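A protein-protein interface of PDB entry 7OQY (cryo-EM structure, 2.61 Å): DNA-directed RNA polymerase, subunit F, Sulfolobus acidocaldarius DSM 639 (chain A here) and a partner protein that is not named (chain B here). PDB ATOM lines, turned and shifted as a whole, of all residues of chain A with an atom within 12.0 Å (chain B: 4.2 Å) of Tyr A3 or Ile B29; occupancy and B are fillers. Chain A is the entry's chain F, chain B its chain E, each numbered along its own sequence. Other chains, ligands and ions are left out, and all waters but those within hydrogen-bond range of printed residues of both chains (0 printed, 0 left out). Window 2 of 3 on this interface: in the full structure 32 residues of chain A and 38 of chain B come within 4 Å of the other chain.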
ATOM      1  N   MET A   1      12.846  13.241  24.989  1.00  0.00           N
ATOM      2  CA  MET A   1      14.163  13.842  25.157  1.00  0.00           C
ATOM      3  C   MET A   1      14.647  13.688  26.595  1.00  0.00           C
ATOM      4  O   MET A   1      14.442  14.572  27.425  1.00  0.00           O
ATOM      5  CB  MET A   1      14.131  15.320  24.764  1.00  0.00           C
ATOM      6  CG  MET A   1      13.835  15.572  23.292  1.00  0.00           C
ATOM      7  SD  MET A   1      14.828  14.547  22.190  1.00  0.00           S
ATOM      8  CE  MET A   1      14.294  15.148  20.591  1.00  0.00           C
ATOM      9  N   SER A   2      15.294  12.561  26.883  1.00  0.00           N
ATOM     10  CA  SER A   2      15.787  12.251  28.217  1.00  0.00           C
ATOM     11  C   SER A   2      17.308  12.267  28.208  1.00  0.00           C
ATOM     12  O   SER A   2      17.935  11.642  27.347  1.00  0.00           O
ATOM     13  CB  SER A   2      15.271  10.890  28.692  1.00  0.00           C
ATOM     14  OG  SER A   2      13.863  10.909  28.858  1.00  0.00           O
ATOM     15  N   TYR A   3      17.894  12.980  29.168  1.00  0.00           N
ATOM     16  CA  TYR A   3      19.335  13.167  29.247  1.00  0.00           C
ATOM     17  C   TYR A   3      19.801  12.958  30.681  1.00  0.00           C
ATOM     18  O   TYR A   3      19.024  13.074  31.633  1.00  0.00           O
ATOM     19  CB  TYR A   3      19.751  14.568  28.760  1.00  0.00           C
ATOM     20  CG  TYR A   3      19.200  14.949  27.403  1.00  0.00           C
ATOM     21  CD1 TYR A   3      17.900  15.416  27.261  1.00  0.00           C
ATOM     22  CD2 TYR A   3      19.986  14.854  26.263  1.00  0.00           C
ATOM     23  CE1 TYR A   3      17.396  15.763  26.023  1.00  0.00           C
ATOM     24  CE2 TYR A   3      19.491  15.198  25.022  1.00  0.00           C
ATOM     25  CZ  TYR A   3      18.197  15.652  24.907  1.00  0.00           C
ATOM     26  OH  TYR A   3      17.699  15.998  23.672  1.00  0.00           O
ATOM     27  N   SER A   4      21.087  12.640  30.823  1.00  0.00           N
ATOM     28  CA  SER A   4      21.721  12.473  32.127  1.00  0.00           C
ATOM     29  C   SER A   4      22.704  13.588  32.454  1.00  0.00           C
ATOM     30  O   SER A   4      22.636  14.165  33.543  1.00  0.00           O
ATOM     31  CB  SER A   4      22.440  11.123  32.198  1.00  0.00           C
ATOM     32  OG  SER A   4      21.531  10.075  32.488  1.00  0.00           O
ATOM     33  N   LEU A   5      23.619  13.894  31.532  1.00  0.00           N
ATOM     34  CA  LEU A   5      24.561  15.008  31.667  1.00  0.00           C
ATOM     35  C   LEU A   5      25.461  14.847  32.892  1.00  0.00           C
ATOM     36  O   LEU A   5      25.456  15.672  33.810  1.00  0.00           O
ATOM     37  CB  LEU A   5      23.823  16.350  31.702  1.00  0.00           C
ATOM     38  CG  LEU A   5      24.645  17.571  31.287  1.00  0.00           C
ATOM     39  CD1 LEU A   5      25.309  17.338  29.939  1.00  0.00           C
ATOM     40  CD2 LEU A   5      23.779  18.817  31.257  1.00  0.00           C
ATOM     41  N   LYS A   6      26.234  13.767  32.907  1.00  0.00           N
ATOM     42  CA  LYS A   6      27.280  13.611  33.904  1.00  0.00           C
ATOM     43  C   LYS A   6      28.617  14.087  33.344  1.00  0.00           C
ATOM     44  O   LYS A   6      28.910  13.941  32.155  1.00  0.00           O
ATOM     45  CB  LYS A   6      27.385  12.155  34.360  1.00  0.00           C
ATOM     46  CG  LYS A   6      26.546  11.832  35.585  1.00  0.00           C
ATOM     47  CD  LYS A   6      26.877  10.457  36.141  1.00  0.00           C
ATOM     48  CE  LYS A   6      26.038  10.144  37.371  1.00  0.00           C
ATOM     49  NZ  LYS A   6      25.854   8.679  37.567  1.00  0.00           N
ATOM     50  N   THR A   7      29.435  14.661  34.221  1.00  0.00           N
ATOM     51  CA  THR A   7      30.704  15.265  33.835  1.00  0.00           C
ATOM     52  C   THR A   7      31.861  14.409  34.334  1.00  0.00           C
ATOM     53  O   THR A   7      31.775  13.803  35.408  1.00  0.00           O
ATOM     54  CB  THR A   7      30.820  16.695  34.375  1.00  0.00           C
ATOM     55  OG1 THR A   7      32.025  17.299  33.890  1.00  0.00           O
ATOM     56  CG2 THR A   7      30.818  16.710  35.899  1.00  0.00           C
ATOM     57  N   GLY A  29      29.698  25.947  13.431  1.00  0.00           N
ATOM     58  CA  GLY A  29      28.426  25.924  14.133  1.00  0.00           C
ATOM     59  C   GLY A  29      27.507  27.060  13.726  1.00  0.00           C
ATOM     60  O   GLY A  29      26.290  26.878  13.627  1.00  0.00           O
ATOM     61  N   ILE B  10      22.696  10.650  27.518  1.00  0.00           N
ATOM     62  CA  ILE B  10      21.801   9.919  26.627  1.00  0.00           C
ATOM     63  C   ILE B  10      21.140  10.922  25.693  1.00  0.00           C
ATOM     64  O   ILE B  10      20.576  11.922  26.148  1.00  0.00           O
ATOM     65  CB  ILE B  10      20.742   9.131  27.418  1.00  0.00           C
ATOM     66  CG1 ILE B  10      21.407   8.135  28.367  1.00  0.00           C
ATOM     67  CG2 ILE B  10      19.806   8.406  26.472  1.00  0.00           C
ATOM     68  CD1 ILE B  10      22.246   7.101  27.669  1.00  0.00           C
ATOM     69  N   VAL B  11      21.203  10.652  24.392  1.00  0.00           N
ATOM     70  CA  VAL B  11      20.603  11.510  23.375  1.00  0.00           C
ATOM     71  C   VAL B  11      19.539  10.716  22.628  1.00  0.00           C
ATOM     72  O   VAL B  11      19.751   9.551  22.271  1.00  0.00           O
ATOM     73  CB  VAL B  11      21.669  12.075  22.413  1.00  0.00           C
ATOM     74  CG1 VAL B  11      22.471  10.955  21.768  1.00  0.00           C
ATOM     75  CG2 VAL B  11      21.026  12.961  21.357  1.00  0.00           C
ATOM     76  N   ILE B  25      23.296  14.036  13.722  1.00  0.00           N
ATOM     77  CA  ILE B  25      22.022  14.232  14.404  1.00  0.00           C
ATOM     78  C   ILE B  25      22.239  14.422  15.898  1.00  0.00           C
ATOM     79  O   ILE B  25      21.564  15.236  16.538  1.00  0.00           O
ATOM     80  CB  ILE B  25      21.071  13.059  14.112  1.00  0.00           C
ATOM     81  CG1 ILE B  25      21.102  12.707  12.625  1.00  0.00           C
ATOM     82  CG2 ILE B  25      19.658  13.395  14.561  1.00  0.00           C
ATOM     83  CD1 ILE B  25      20.606  13.817  11.728  1.00  0.00           C
ATOM     84  N   ALA B  26      23.176  13.672  16.481  1.00  0.00           N
ATOM     85  CA  ALA B  26      23.440  13.794  17.910  1.00  0.00           C
ATOM     86  C   ALA B  26      23.960  15.181  18.258  1.00  0.00           C
ATOM     87  O   ALA B  26      23.502  15.795  19.230  1.00  0.00           O
ATOM     88  CB  ALA B  26      24.433  12.721  18.353  1.00  0.00           C
ATOM     89  N   ILE B  27      24.909  15.698  17.474  1.00  0.00           N
ATOM     90  CA  ILE B  27      25.440  17.027  17.762  1.00  0.00           C
ATOM     91  C   ILE B  27      24.379  18.092  17.509  1.00  0.00           C
ATOM     92  O   ILE B  27      24.299  19.088  18.237  1.00  0.00           O
ATOM     93  CB  ILE B  27      26.737  17.287  16.968  1.00  0.00           C
ATOM     94  CG1 ILE B  27      27.471  18.503  17.534  1.00  0.00           C
ATOM     95  CG2 ILE B  27      26.464  17.487  15.490  1.00  0.00           C
ATOM     96  CD1 ILE B  27      28.904  18.617  17.068  1.00  0.00           C
ATOM     97  N   LYS B  28      23.529  17.892  16.495  1.00  0.00           N
ATOM     98  CA  LYS B  28      22.439  18.833  16.254  1.00  0.00           C
ATOM     99  C   LYS B  28      21.477  18.879  17.436  1.00  0.00           C
ATOM    100  O   LYS B  28      21.095  19.964  17.891  1.00  0.00           O
ATOM    101  CB  LYS B  28      21.698  18.457  14.971  1.00  0.00           C
ATOM    102  CG  LYS B  28      20.487  19.323  14.676  1.00  0.00           C
ATOM    103  CD  LYS B  28      19.766  18.856  13.421  1.00  0.00           C
ATOM    104  CE  LYS B  28      20.664  18.959  12.198  1.00  0.00           C
ATOM    105  NZ  LYS B  28      20.289  17.973  11.147  1.00  0.00           N
ATOM    106  N   ILE B  29      21.081  17.713  17.950  1.00  0.00           N
ATOM    107  CA  ILE B  29      20.165  17.663  19.087  1.00  0.00           C
ATOM    108  C   ILE B  29      20.814  18.269  20.323  1.00  0.00           C
ATOM    109  O   ILE B  29      20.175  19.009  21.082  1.00  0.00           O
ATOM    110  CB  ILE B  29      19.702  16.214  19.338  1.00  0.00           C
ATOM    111  CG1 ILE B  29      18.878  15.699  18.157  1.00  0.00           C
ATOM    112  CG2 ILE B  29      18.901  16.121  20.628  1.00  0.00           C
ATOM    113  CD1 ILE B  29      17.467  16.242  18.105  1.00  0.00           C
ATOM    114  N   LEU B  30      22.097  17.971  20.544  1.00  0.00           N
ATOM    115  CA  LEU B  30      22.804  18.531  21.691  1.00  0.00           C
ATOM    116  C   LEU B  30      22.858  20.052  21.613  1.00  0.00           C
ATOM    117  O   LEU B  30      22.666  20.742  22.620  1.00  0.00           O
ATOM    118  CB  LEU B  30      24.212  17.943  21.775  1.00  0.00           C
ATOM    119  CG  LEU B  30      24.320  16.558  22.410  1.00  0.00           C
ATOM    120  CD1 LEU B  30      25.759  16.075  22.401  1.00  0.00           C
ATOM    121  CD2 LEU B  30      23.765  16.576  23.824  1.00  0.00           C
ATOM    122  N   ARG B  31      23.124  20.593  20.422  1.00  0.00           N
ATOM    123  CA  ARG B  31      23.162  22.043  20.264  1.00  0.00           C
ATOM    124  C   ARG B  31      21.782  22.653  20.479  1.00  0.00           C
ATOM    125  O   ARG B  31      21.640  23.668  21.170  1.00  0.00           O
ATOM    126  CB  ARG B  31      23.710  22.404  18.883  1.00  0.00           C
ATOM    127  CG  ARG B  31      25.196  22.121  18.725  1.00  0.00           C
ATOM    128  CD  ARG B  31      25.898  23.201  17.925  1.00  0.00           C
ATOM    129  NE  ARG B  31      27.295  22.864  17.683  1.00  0.00           N
ATOM    130  CZ  ARG B  31      27.749  22.315  16.565  1.00  0.00           C
ATOM    131  NH1 ARG B  31      26.943  22.040  15.552  1.00  0.00           N
ATOM    132  NH2 ARG B  31      29.045  22.032  16.460  1.00  0.00           N
ATOM    133  N   GLN B  32      20.745  22.041  19.902  1.00  0.00           N
ATOM    134  CA  GLN B  32      19.392  22.556  20.083  1.00  0.00           C
ATOM    135  C   GLN B  32      18.900  22.427  21.519  1.00  0.00           C
ATOM    136  O   GLN B  32      17.946  23.116  21.895  1.00  0.00           O
ATOM    137  CB  GLN B  32      18.416  21.843  19.145  1.00  0.00           C
ATOM    138  CG  GLN B  32      18.748  21.965  17.671  1.00  0.00           C
ATOM    139  CD  GLN B  32      17.588  21.564  16.782  1.00  0.00           C
ATOM    140  OE1 GLN B  32      16.471  21.357  17.255  1.00  0.00           O
ATOM    141  NE2 GLN B  32      17.848  21.450  15.484  1.00  0.00           N
ATOM    142  N   GLU B  33      19.517  21.564  22.327  1.00  0.00           N
ATOM    143  CA  GLU B  33      19.046  21.325  23.682  1.00  0.00           C
ATOM    144  C   GLU B  33      19.961  21.890  24.764  1.00  0.00           C
ATOM    145  O   GLU B  33      19.534  21.987  25.919  1.00  0.00           O
ATOM    146  CB  GLU B  33      18.853  19.816  23.910  1.00  0.00           C
ATOM    147  CG  GLU B  33      17.871  19.461  25.018  1.00  0.00           C
ATOM    148  CD  GLU B  33      18.562  19.134  26.324  1.00  0.00           C
ATOM    149  OE1 GLU B  33      19.706  18.639  26.280  1.00  0.00           O
ATOM    150  OE2 GLU B  33      17.960  19.371  27.394  1.00  0.00           O
ATOM    151  N   TYR B  34      21.192  22.282  24.428  1.00  0.00           N
ATOM    152  CA  TYR B  34      22.139  22.758  25.426  1.00  0.00           C
ATOM    153  C   TYR B  34      22.743  24.123  25.124  1.00  0.00           C
ATOM    154  O   TYR B  34      23.494  24.639  25.960  1.00  0.00           O
ATOM    155  CB  TYR B  34      23.279  21.744  25.607  1.00  0.00           C
ATOM    156  CG  TYR B  34      22.923  20.585  26.510  1.00  0.00           C
ATOM    157  CD1 TYR B  34      22.018  20.745  27.550  1.00  0.00           C
ATOM    158  CD2 TYR B  34      23.478  19.328  26.312  1.00  0.00           C
ATOM    159  CE1 TYR B  34      21.686  19.689  28.377  1.00  0.00           C
ATOM    160  CE2 TYR B  34      23.151  18.266  27.131  1.00  0.00           C
ATOM    161  CZ  TYR B  34      22.252  18.450  28.160  1.00  0.00           C
ATOM    162  OH  TYR B  34      21.923  17.395  28.978  1.00  0.00           O
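The side-chain hydroxyl (OH) of Tyr A3 sits at hydrogen-bond distance from the side-chain sulfur (SD) of Met A1, at 3.5 Å.
The backbone carbonyl oxygen of Ser A2 sits close to the backbone carbonyl oxygen of Ile B10 (2.9 Å).
Met A1 touches none of the printed residues of chain B. Of the printed residues of chain B, Ser A2 touches Ile B10. Tyr A3 touches just these residues of chain B: Ile B10, Ile B29, Glu B33 and Tyr B34. Ser A4 touches none of the printed residues of chain B. Of the printed residues of chain B, Leu A5 touches Tyr B34 (3.3 Å). Ile B10 touches just these residues of chain A: Ser A2 and Tyr A3. Ile B27 touches none of the printed residues of chain A. Lys B28 touches none of the printed residues of chain A. Leu B30 touches none of the printed residues of chain A. No residue of chain A comes within 4 Å of Gln B32. Of the printed residues of chain A, Tyr B34 touches Tyr A3 (3.6 Å) and Leu A5 (3.3 Å). The nearest printed residue of chain B that does not touch Tyr A3 is Val B11 (4.2 Å). The nearest residue of chain A that does not touch Ile B29 is Met A1 (4.2 Å). The nearest printed residue of chain B that does not touch Leu A5 is Ile B10 (5.2 Å).
O of Ile B10 touches CD2 of Tyr A3 (3.0 Å). OH of Tyr A3 touches CG2 of Ile B29, at 3.3 Å. CD of Glu B33 touches CE1 of Tyr A3 (3.6 Å). OH of Tyr B34 touches CB of Tyr A3, at 3.6 Å. CD2 of Leu A5 touches OH of Tyr B34, at 3.3 Å.
Printed residues of chain B that touch a printed residue of chain A: Ile B10, Ile B29, Glu B33 and Tyr B34. Hydrophobic or aromatic side chains of chain B within 4 Å of the printed part of chain A: Ile B10, Ile B29 and Tyr B34. Of the 8 printed residues of chain A, 3 touch a printed residue of chain B. Printed residues of chain A that touch a printed residue of chain B: Ser A2, Tyr A3 and Leu A5. Hydrophobic or aromatic side chains of chain A within 4 Å of the printed part of chain B: Tyr A3 and Leu A5. Along chain A the printed residues that touch a printed residue of chain B span positions 2 to 5. Among the printed residues, 6 pairs touch across the chains.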
